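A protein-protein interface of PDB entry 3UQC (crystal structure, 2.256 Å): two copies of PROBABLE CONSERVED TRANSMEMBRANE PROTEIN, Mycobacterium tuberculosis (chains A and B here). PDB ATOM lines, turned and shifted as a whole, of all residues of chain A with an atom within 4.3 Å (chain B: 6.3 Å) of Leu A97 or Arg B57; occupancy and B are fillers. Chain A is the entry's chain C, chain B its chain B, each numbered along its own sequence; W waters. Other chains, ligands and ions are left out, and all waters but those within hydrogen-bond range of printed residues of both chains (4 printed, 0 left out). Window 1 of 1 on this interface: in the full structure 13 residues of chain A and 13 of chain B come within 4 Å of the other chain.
The side-chain carboxylate (OD2) of Asp B52 lies within salt-bridge range of the guanidinium group (NH2) of Arg B32, at 2.8 Å.
O of Arg B32 sits at hydrogen-bond distance from OG1 of Thr B53 (2.7 Å).
The side-chain carboxylate (OD1) of Asp B52 is in hydrogen-bond range of the backbone NH (N) of Leu B55 (3.3 Å).
N of Arg A95 lies within hydrogen-bond range of OE1 of Glu A111 (2.9 Å).
The backbone NH of Leu A97 sits at hydrogen-bond distance from the backbone carbonyl oxygen of Val A109 (2.7 Å).
N of Val A109 is in hydrogen-bond range of O of Asp A98, 2.8 Å away.
Of the 9 printed residues of chain A, 5 touch a printed residue of chain B.
Printed residues of chain B that touch a printed residue of chain A: Arg B32, Leu B55, Arg B57, Arg B95 and Val B96.
Hydrophobic or aromatic side chains of chain B within 4 Å of the printed part of chain A: Leu B55.
Among the printed residues, 8 pairs touch across the chains.
Among the printed residues, Asp or Glu carboxylates within 4 Å of a Lys or Arg side-chain nitrogen of the other chain: Asp A98 with Arg B32 (3.1 Å) and Glu A111 with Arg B95 (3.4 Å).
The guanidinium group of Arg B32 lies within salt-bridge range of the side-chain carboxylate of Asp A98 (3.1 Å).
NH2 of Arg B57 is in hydrogen-bond range of O of Leu A97 (3.0 Å).
The guanidinium group (NH2) of Arg B95 lies within salt-bridge range of the side-chain carboxylate (OE2) of Glu A111 (3.4 Å).
The guanidinium group (NH2) of Arg A57 is in hydrogen-bond range of the backbone carbonyl oxygen (O) of Val B96.
Arg A95 touches Arg B95.
O of Leu A97 touches CD2 of Leu B55, at 3.7 Å.
Leu A97 touches Arg B95.
Asp A98 touches Leu B55 (OD1 to CD1, 3.6 Å).
Water W2 lies within hydrogen-bond range of NE of Arg B57 and O of Val A96.
Water W1 lies within hydrogen-bond range of N of Val B96 (3.0 Å) and NH1 of Arg A57 (3.5 Å).
Water W3 lies within hydrogen-bond range of NE of Arg B95 and NE of Arg A95.
Water W4 lies within hydrogen-bond range of the guanidinium group of Arg B32 (3.1 Å) and the backbone carbonyl oxygen of Leu A97 (3.4 Å).
Of chain B, only Leu B55 (3.7 Å), Arg B57 (3.0 Å) and Arg B95 (3.7 Å) come within 4 Å of Leu A97.
Of the printed residues of chain A, Arg B57 touches Leu A97.
Printed residues of chain A within 4 Å of Leu B55: Leu A97 (3.7 Å) and Asp A98 (3.6 Å).
Printed residues of chain B within 4 Å of Glu A111: Arg B95 (3.4 Å).
Of the printed residues of chain A, Val B96 touches Arg A57.
Of the printed residues of chain B, Arg A95 touches Arg B95 (3.7 Å).
Tyr B33 touches none of the printed residues of chain A.
Ala B50 touches none of the printed residues of chain A.
The nearest printed residue of chain B that does not touch Arg A95 is Arg B57 (4.8 Å).
Arg A57 touches Val B96, but with the chains exchanged Val A96 does not touch Arg B57 (4.1 Å).
Arg B95 touches its own counterpart, Arg A95.
Leu A97 touches Arg B57, but with the chains exchanged Arg A57 does not touch Leu B97 (4.4 Å).
Leu A97 touches Arg B95, but with the chains exchanged Arg A95 does not touch Leu B97 (6.5 Å).
Positions printed for both chains: 57, 59, 95, 96 and 97.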
ATOM      1  N   ARG A  57      13.978 -27.099 -13.640  1.00  0.00           N
ATOM      2  CA  ARG A  57      13.819 -26.177 -14.760  1.00  0.00           C
ATOM      3  C   ARG A  57      13.262 -24.838 -14.287  1.00  0.00           C
ATOM      4  O   ARG A  57      12.634 -24.748 -13.234  1.00  0.00           O
ATOM      5  CB  ARG A  57      12.933 -26.781 -15.857  1.00  0.00           C
ATOM      6  CG  ARG A  57      11.518 -27.109 -15.414  1.00  0.00           C
ATOM      7  CD  ARG A  57      10.506 -26.227 -16.127  1.00  0.00           C
ATOM      8  NE  ARG A  57       9.129 -26.538 -15.753  1.00  0.00           N
ATOM      9  CZ  ARG A  57       8.430 -27.553 -16.258  1.00  0.00           C
ATOM     10  NH1 ARG A  57       8.986 -28.364 -17.150  1.00  0.00           N
ATOM     11  NH2 ARG A  57       7.181 -27.762 -15.866  1.00  0.00           N
ATOM     12  N   VAL A  59      11.054 -21.372 -14.038  1.00  0.00           N
ATOM     13  CA  VAL A  59       9.667 -20.964 -14.184  1.00  0.00           C
ATOM     14  C   VAL A  59       9.543 -19.486 -13.859  1.00  0.00           C
ATOM     15  O   VAL A  59      10.398 -18.920 -13.179  1.00  0.00           O
ATOM     16  CB  VAL A  59       8.745 -21.752 -13.234  1.00  0.00           C
ATOM     17  CG1 VAL A  59       8.714 -23.229 -13.615  1.00  0.00           C
ATOM     18  CG2 VAL A  59       9.191 -21.581 -11.791  1.00  0.00           C
ATOM     19  N   ARG A  95       2.364 -20.208 -20.403  1.00  0.00           N
ATOM     20  CA  ARG A  95       1.513 -21.315 -19.994  1.00  0.00           C
ATOM     21  C   ARG A  95       1.466 -21.368 -18.475  1.00  0.00           C
ATOM     22  O   ARG A  95       2.510 -21.406 -17.826  1.00  0.00           O
ATOM     23  CB  ARG A  95       2.091 -22.630 -20.518  1.00  0.00           C
ATOM     24  CG  ARG A  95       1.163 -23.824 -20.395  1.00  0.00           C
ATOM     25  CD  ARG A  95       0.179 -23.869 -21.555  1.00  0.00           C
ATOM     26  NE  ARG A  95      -0.551 -25.134 -21.609  1.00  0.00           N
ATOM     27  CZ  ARG A  95      -1.818 -25.282 -21.237  1.00  0.00           C
ATOM     28  NH1 ARG A  95      -2.505 -24.241 -20.787  1.00  0.00           N
ATOM     29  NH2 ARG A  95      -2.401 -26.470 -21.321  1.00  0.00           N
ATOM     30  N   VAL A  96       0.266 -21.385 -17.903  1.00  0.00           N
ATOM     31  CA  VAL A  96       0.163 -21.459 -16.457  1.00  0.00           C
ATOM     32  C   VAL A  96       0.370 -22.903 -16.040  1.00  0.00           C
ATOM     33  O   VAL A  96      -0.412 -23.782 -16.392  1.00  0.00           O
ATOM     34  CB  VAL A  96      -1.219 -20.989 -15.970  1.00  0.00           C
ATOM     35  CG1 VAL A  96      -1.362 -21.208 -14.473  1.00  0.00           C
ATOM     36  CG2 VAL A  96      -1.436 -19.528 -16.324  1.00  0.00           C
ATOM     37  N   LEU A  97       1.437 -23.137 -15.286  1.00  0.00           N
ATOM     38  CA  LEU A  97       1.773 -24.467 -14.800  1.00  0.00           C
ATOM     39  C   LEU A  97       1.006 -24.847 -13.541  1.00  0.00           C
ATOM     40  O   LEU A  97       0.728 -26.022 -13.305  1.00  0.00           O
ATOM     41  CB  LEU A  97       3.277 -24.587 -14.585  1.00  0.00           C
ATOM     42  CG  LEU A  97       4.067 -24.158 -15.822  1.00  0.00           C
ATOM     43  CD1 LEU A  97       5.559 -24.395 -15.619  1.00  0.00           C
ATOM     44  CD2 LEU A  97       3.547 -24.884 -17.057  1.00  0.00           C
ATOM     45  N   ASP A  98       0.647 -23.846 -12.743  1.00  0.00           N
ATOM     46  CA  ASP A  98      -0.019 -24.110 -11.481  1.00  0.00           C
ATOM     47  C   ASP A  98      -0.396 -22.817 -10.774  1.00  0.00           C
ATOM     48  O   ASP A  98       0.160 -21.753 -11.037  1.00  0.00           O
ATOM     49  CB  ASP A  98       0.935 -24.898 -10.579  1.00  0.00           C
ATOM     50  CG  ASP A  98       0.212 -25.762  -9.566  1.00  0.00           C
ATOM     51  OD1 ASP A  98      -1.018 -25.603  -9.397  1.00  0.00           O
ATOM     52  OD2 ASP A  98       0.884 -26.607  -8.936  1.00  0.00           O
ATOM     53  N   VAL A 109       2.395 -20.025 -10.999  1.00  0.00           N
ATOM     54  CA  VAL A 109       3.601 -20.562 -11.625  1.00  0.00           C
ATOM     55  C   VAL A 109       3.379 -20.748 -13.122  1.00  0.00           C
ATOM     56  O   VAL A 109       2.436 -21.415 -13.535  1.00  0.00           O
ATOM     57  CB  VAL A 109       4.007 -21.916 -11.016  1.00  0.00           C
ATOM     58  CG1 VAL A 109       5.375 -22.344 -11.543  1.00  0.00           C
ATOM     59  CG2 VAL A 109       4.011 -21.839  -9.491  1.00  0.00           C
ATOM     60  N   ALA A 110       4.246 -20.149 -13.929  1.00  0.00           N
ATOM     61  CA  ALA A 110       4.140 -20.252 -15.376  1.00  0.00           C
ATOM     62  C   ALA A 110       5.475 -20.685 -15.978  1.00  0.00           C
ATOM     63  O   ALA A 110       6.507 -20.633 -15.313  1.00  0.00           O
ATOM     64  CB  ALA A 110       3.695 -18.933 -15.965  1.00  0.00           C
ATOM     65  N   GLU A 111       5.446 -21.120 -17.236  1.00  0.00           N
ATOM     66  CA  GLU A 111       6.661 -21.505 -17.939  1.00  0.00           C
ATOM     67  C   GLU A 111       7.577 -20.297 -18.019  1.00  0.00           C
ATOM     68  O   GLU A 111       7.104 -19.160 -18.041  1.00  0.00           O
ATOM     69  CB  GLU A 111       6.339 -21.982 -19.360  1.00  0.00           C
ATOM     70  CG  GLU A 111       5.786 -20.875 -20.260  1.00  0.00           C
ATOM     71  CD  GLU A 111       5.521 -21.336 -21.687  1.00  0.00           C
ATOM     72  OE1 GLU A 111       4.421 -21.053 -22.213  1.00  0.00           O
ATOM     73  OE2 GLU A 111       6.414 -21.970 -22.287  1.00  0.00           O
ATOM     74  N   ARG B  32      -5.476 -34.572  -5.742  1.00  0.00           N
ATOM     75  CA  ARG B  32      -5.400 -33.588  -6.819  1.00  0.00           C
ATOM     76  C   ARG B  32      -5.910 -34.099  -8.162  1.00  0.00           C
ATOM     77  O   ARG B  32      -6.694 -33.427  -8.833  1.00  0.00           O
ATOM     78  CB  ARG B  32      -3.985 -33.036  -6.982  1.00  0.00           C
ATOM     79  CG  ARG B  32      -3.880 -32.132  -8.193  1.00  0.00           C
ATOM     80  CD  ARG B  32      -2.676 -31.218  -8.150  1.00  0.00           C
ATOM     81  NE  ARG B  32      -2.706 -30.289  -9.274  1.00  0.00           N
ATOM     82  CZ  ARG B  32      -1.840 -29.298  -9.450  1.00  0.00           C
ATOM     83  NH1 ARG B  32      -0.869 -29.104  -8.569  1.00  0.00           N
ATOM     84  NH2 ARG B  32      -1.945 -28.503 -10.507  1.00  0.00           N
ATOM     85  N   TYR B  33      -5.462 -35.284  -8.562  1.00  0.00           N
ATOM     86  CA  TYR B  33      -5.845 -35.824  -9.860  1.00  0.00           C
ATOM     87  C   TYR B  33      -6.947 -36.867  -9.760  1.00  0.00           C
ATOM     88  O   TYR B  33      -6.974 -37.671  -8.829  1.00  0.00           O
ATOM     89  CB  TYR B  33      -4.625 -36.394 -10.583  1.00  0.00           C
ATOM     90  CG  TYR B  33      -3.469 -35.430 -10.606  1.00  0.00           C
ATOM     91  CD1 TYR B  33      -3.484 -34.323 -11.443  1.00  0.00           C
ATOM     92  CD2 TYR B  33      -2.370 -35.615  -9.781  1.00  0.00           C
ATOM     93  CE1 TYR B  33      -2.436 -33.427 -11.463  1.00  0.00           C
ATOM     94  CE2 TYR B  33      -1.312 -34.720  -9.793  1.00  0.00           C
ATOM     95  CZ  TYR B  33      -1.350 -33.631 -10.640  1.00  0.00           C
ATOM     96  OH  TYR B  33      -0.302 -32.740 -10.662  1.00  0.00           O
ATOM     97  N   ALA B  50      -6.597 -37.965 -17.205  1.00  0.00           N
ATOM     98  CA  ALA B  50      -7.159 -37.559 -15.916  1.00  0.00           C
ATOM     99  C   ALA B  50      -7.594 -36.093 -15.827  1.00  0.00           C
ATOM    100  O   ALA B  50      -7.269 -35.272 -16.686  1.00  0.00           O
ATOM    101  CB  ALA B  50      -6.190 -37.889 -14.786  1.00  0.00           C
ATOM    102  N   LEU B  51      -8.347 -35.785 -14.775  1.00  0.00           N
ATOM    103  CA  LEU B  51      -8.736 -34.409 -14.481  1.00  0.00           C
ATOM    104  C   LEU B  51      -7.883 -33.855 -13.349  1.00  0.00           C
ATOM    105  O   LEU B  51      -7.775 -34.466 -12.286  1.00  0.00           O
ATOM    106  CB  LEU B  51     -10.216 -34.331 -14.085  1.00  0.00           C
ATOM    107  CG  LEU B  51     -10.715 -32.942 -13.668  1.00  0.00           C
ATOM    108  CD1 LEU B  51     -10.668 -31.975 -14.846  1.00  0.00           C
ATOM    109  CD2 LEU B  51     -12.125 -33.010 -13.079  1.00  0.00           C
ATOM    110  N   ASP B  52      -7.299 -32.683 -13.558  1.00  0.00           N
ATOM    111  CA  ASP B  52      -6.570 -32.042 -12.479  1.00  0.00           C
ATOM    112  C   ASP B  52      -7.611 -31.167 -11.803  1.00  0.00           C
ATOM    113  O   ASP B  52      -8.013 -30.138 -12.341  1.00  0.00           O
ATOM    114  CB  ASP B  52      -5.444 -31.183 -13.060  1.00  0.00           C
ATOM    115  CG  ASP B  52      -4.742 -30.325 -12.012  1.00  0.00           C
ATOM    116  OD1 ASP B  52      -5.221 -30.228 -10.861  1.00  0.00           O
ATOM    117  OD2 ASP B  52      -3.702 -29.730 -12.353  1.00  0.00           O
ATOM    118  N   THR B  53      -8.011 -31.560 -10.597  1.00  0.00           N
ATOM    119  CA  THR B  53      -9.179 -30.966  -9.959  1.00  0.00           C
ATOM    120  C   THR B  53      -8.855 -29.609  -9.362  1.00  0.00           C
ATOM    121  O   THR B  53      -9.755 -28.849  -9.020  1.00  0.00           O
ATOM    122  CB  THR B  53      -9.765 -31.874  -8.861  1.00  0.00           C
ATOM    123  OG1 THR B  53      -8.808 -32.037  -7.807  1.00  0.00           O
ATOM    124  CG2 THR B  53     -10.130 -33.236  -9.433  1.00  0.00           C
ATOM    125  N   ALA B  54      -7.564 -29.319  -9.233  1.00  0.00           N
ATOM    126  CA  ALA B  54      -7.112 -28.036  -8.716  1.00  0.00           C
ATOM    127  C   ALA B  54      -7.159 -26.942  -9.776  1.00  0.00           C
ATOM    128  O   ALA B  54      -7.589 -25.820  -9.508  1.00  0.00           O
ATOM    129  CB  ALA B  54      -5.701 -28.165  -8.155  1.00  0.00           C
ATOM    130  N   LEU B  55      -6.692 -27.265 -10.976  1.00  0.00           N
ATOM    131  CA  LEU B  55      -6.673 -26.301 -12.072  1.00  0.00           C
ATOM    132  C   LEU B  55      -7.854 -26.444 -13.024  1.00  0.00           C
ATOM    133  O   LEU B  55      -7.977 -25.688 -13.987  1.00  0.00           O
ATOM    134  CB  LEU B  55      -5.349 -26.378 -12.832  1.00  0.00           C
ATOM    135  CG  LEU B  55      -4.257 -25.421 -12.338  1.00  0.00           C
ATOM    136  CD1 LEU B  55      -4.306 -25.250 -10.827  1.00  0.00           C
ATOM    137  CD2 LEU B  55      -2.885 -25.891 -12.779  1.00  0.00           C
ATOM    138  N   ASP B  56      -8.711 -27.423 -12.753  1.00  0.00           N
ATOM    139  CA  ASP B  56      -9.820 -27.749 -13.645  1.00  0.00           C
ATOM    140  C   ASP B  56      -9.338 -27.894 -15.088  1.00  0.00           C
ATOM    141  O   ASP B  56      -9.846 -27.243 -16.000  1.00  0.00           O
ATOM    142  CB  ASP B  56     -10.952 -26.719 -13.540  1.00  0.00           C
ATOM    143  CG  ASP B  56     -12.270 -27.243 -14.096  1.00  0.00           C
ATOM    144  OD1 ASP B  56     -12.479 -28.474 -14.069  1.00  0.00           O
ATOM    145  OD2 ASP B  56     -13.098 -26.429 -14.557  1.00  0.00           O
ATOM    146  N   ARG B  57      -8.328 -28.733 -15.283  1.00  0.00           N
ATOM    147  CA  ARG B  57      -7.886 -29.079 -16.624  1.00  0.00           C
ATOM    148  C   ARG B  57      -7.461 -30.538 -16.693  1.00  0.00           C
ATOM    149  O   ARG B  57      -7.179 -31.168 -15.675  1.00  0.00           O
ATOM    150  CB  ARG B  57      -6.758 -28.159 -17.103  1.00  0.00           C
ATOM    151  CG  ARG B  57      -5.486 -28.162 -16.264  1.00  0.00           C
ATOM    152  CD  ARG B  57      -4.343 -27.586 -17.094  1.00  0.00           C
ATOM    153  NE  ARG B  57      -3.150 -27.186 -16.345  1.00  0.00           N
ATOM    154  CZ  ARG B  57      -2.563 -27.897 -15.385  1.00  0.00           C
ATOM    155  NH1 ARG B  57      -3.060 -29.066 -15.005  1.00  0.00           N
ATOM    156  NH2 ARG B  57      -1.472 -27.426 -14.794  1.00  0.00           N
ATOM    157  N   GLN B  58      -7.439 -31.079 -17.902  1.00  0.00           N
ATOM    158  CA  GLN B  58      -6.970 -32.439 -18.095  1.00  0.00           C
ATOM    159  C   GLN B  58      -5.455 -32.477 -18.041  1.00  0.00           C
ATOM    160  O   GLN B  58      -4.786 -31.502 -18.388  1.00  0.00           O
ATOM    161  CB  GLN B  58      -7.441 -32.989 -19.436  1.00  0.00           C
ATOM    162  CG  GLN B  58      -8.941 -33.049 -19.577  1.00  0.00           C
ATOM    163  CD  GLN B  58      -9.374 -34.034 -20.639  1.00  0.00           C
ATOM    164  OE1 GLN B  58      -9.640 -35.197 -20.343  1.00  0.00           O
ATOM    165  NE2 GLN B  58      -9.448 -33.576 -21.883  1.00  0.00           N
ATOM    166  N   VAL B  59      -4.930 -33.612 -17.593  1.00  0.00           N
ATOM    167  CA  VAL B  59      -3.510 -33.902 -17.661  1.00  0.00           C
ATOM    168  C   VAL B  59      -3.343 -35.344 -18.116  1.00  0.00           C
ATOM    169  O   VAL B  59      -4.283 -36.137 -18.022  1.00  0.00           O
ATOM    170  CB  VAL B  59      -2.833 -33.742 -16.289  1.00  0.00           C
ATOM    171  CG1 VAL B  59      -2.774 -32.271 -15.884  1.00  0.00           C
ATOM    172  CG2 VAL B  59      -3.569 -34.568 -15.244  1.00  0.00           C
ATOM    173  N   ARG B  95       4.932 -31.258 -22.306  1.00  0.00           N
ATOM    174  CA  ARG B  95       5.569 -30.676 -21.133  1.00  0.00           C
ATOM    175  C   ARG B  95       5.270 -31.529 -19.906  1.00  0.00           C
ATOM    176  O   ARG B  95       4.127 -31.927 -19.679  1.00  0.00           O
ATOM    177  CB  ARG B  95       5.069 -29.246 -20.905  1.00  0.00           C
ATOM    178  CG  ARG B  95       5.899 -28.455 -19.899  1.00  0.00           C
ATOM    179  CD  ARG B  95       5.145 -27.255 -19.337  1.00  0.00           C
ATOM    180  NE  ARG B  95       4.571 -26.406 -20.378  1.00  0.00           N
ATOM    181  CZ  ARG B  95       5.274 -25.560 -21.125  1.00  0.00           C
ATOM    182  NH1 ARG B  95       6.584 -25.459 -20.958  1.00  0.00           N
ATOM    183  NH2 ARG B  95       4.668 -24.824 -22.048  1.00  0.00           N
ATOM    184  N   VAL B  96       6.303 -31.815 -19.124  1.00  0.00           N
ATOM    185  CA  VAL B  96       6.128 -32.516 -17.858  1.00  0.00           C
ATOM    186  C   VAL B  96       5.771 -31.516 -16.754  1.00  0.00           C
ATOM    187  O   VAL B  96       6.483 -30.532 -16.535  1.00  0.00           O
ATOM    188  CB  VAL B  96       7.402 -33.309 -17.487  1.00  0.00           C
ATOM    189  CG1 VAL B  96       7.297 -33.881 -16.076  1.00  0.00           C
ATOM    190  CG2 VAL B  96       7.652 -34.412 -18.517  1.00  0.00           C
ATOM    191  N   LEU B  97       4.620 -31.726 -16.127  1.00  0.00           N
ATOM    192  CA  LEU B  97       4.161 -30.878 -15.027  1.00  0.00           C
ATOM    193  C   LEU B  97       4.739 -31.247 -13.661  1.00  0.00           C
ATOM    194  O   LEU B  97       5.001 -30.380 -12.832  1.00  0.00           O
ATOM    195  CB  LEU B  97       2.633 -30.841 -14.982  1.00  0.00           C
ATOM    196  CG  LEU B  97       2.028 -30.337 -16.295  1.00  0.00           C
ATOM    197  CD1 LEU B  97       0.502 -30.410 -16.266  1.00  0.00           C
ATOM    198  CD2 LEU B  97       2.517 -28.921 -16.585  1.00  0.00           C
ATOM    199  N   TRP B 112      -1.950 -32.014 -20.981  1.00  0.00           N
ATOM    200  CA  TRP B 112      -2.780 -32.744 -21.922  1.00  0.00           C
ATOM    201  C   TRP B 112      -2.595 -32.188 -23.325  1.00  0.00           C
ATOM    202  O   TRP B 112      -2.604 -30.978 -23.523  1.00  0.00           O
ATOM    203  CB  TRP B 112      -4.257 -32.694 -21.523  1.00  0.00           C
ATOM    204  CG  TRP B 112      -5.109 -33.519 -22.429  1.00  0.00           C
ATOM    205  CD1 TRP B 112      -5.959 -33.068 -23.399  1.00  0.00           C
ATOM    206  CD2 TRP B 112      -5.162 -34.948 -22.484  1.00  0.00           C
ATOM    207  NE1 TRP B 112      -6.552 -34.127 -24.040  1.00  0.00           N
ATOM    208  CE2 TRP B 112      -6.076 -35.293 -23.500  1.00  0.00           C
ATOM    209  CE3 TRP B 112      -4.528 -35.970 -21.769  1.00  0.00           C
ATOM    210  CZ2 TRP B 112      -6.375 -36.620 -23.816  1.00  0.00           C
ATOM    211  CZ3 TRP B 112      -4.823 -37.283 -22.085  1.00  0.00           C
ATOM    212  CH2 TRP B 112      -5.739 -37.597 -23.098  1.00  0.00           C
HETATM  213  O   HOH W   1       8.832 -30.479 -19.900  1.00  0.00           O
HETATM  214  O   HOH W   2      -2.464 -25.084 -17.299  1.00  0.00           O
HETATM  215  O   HOH W   3       1.630 -26.958 -20.480  1.00  0.00           O
HETATM  216  O   HOH W   4       0.857 -29.079 -11.777  1.00  0.00           O
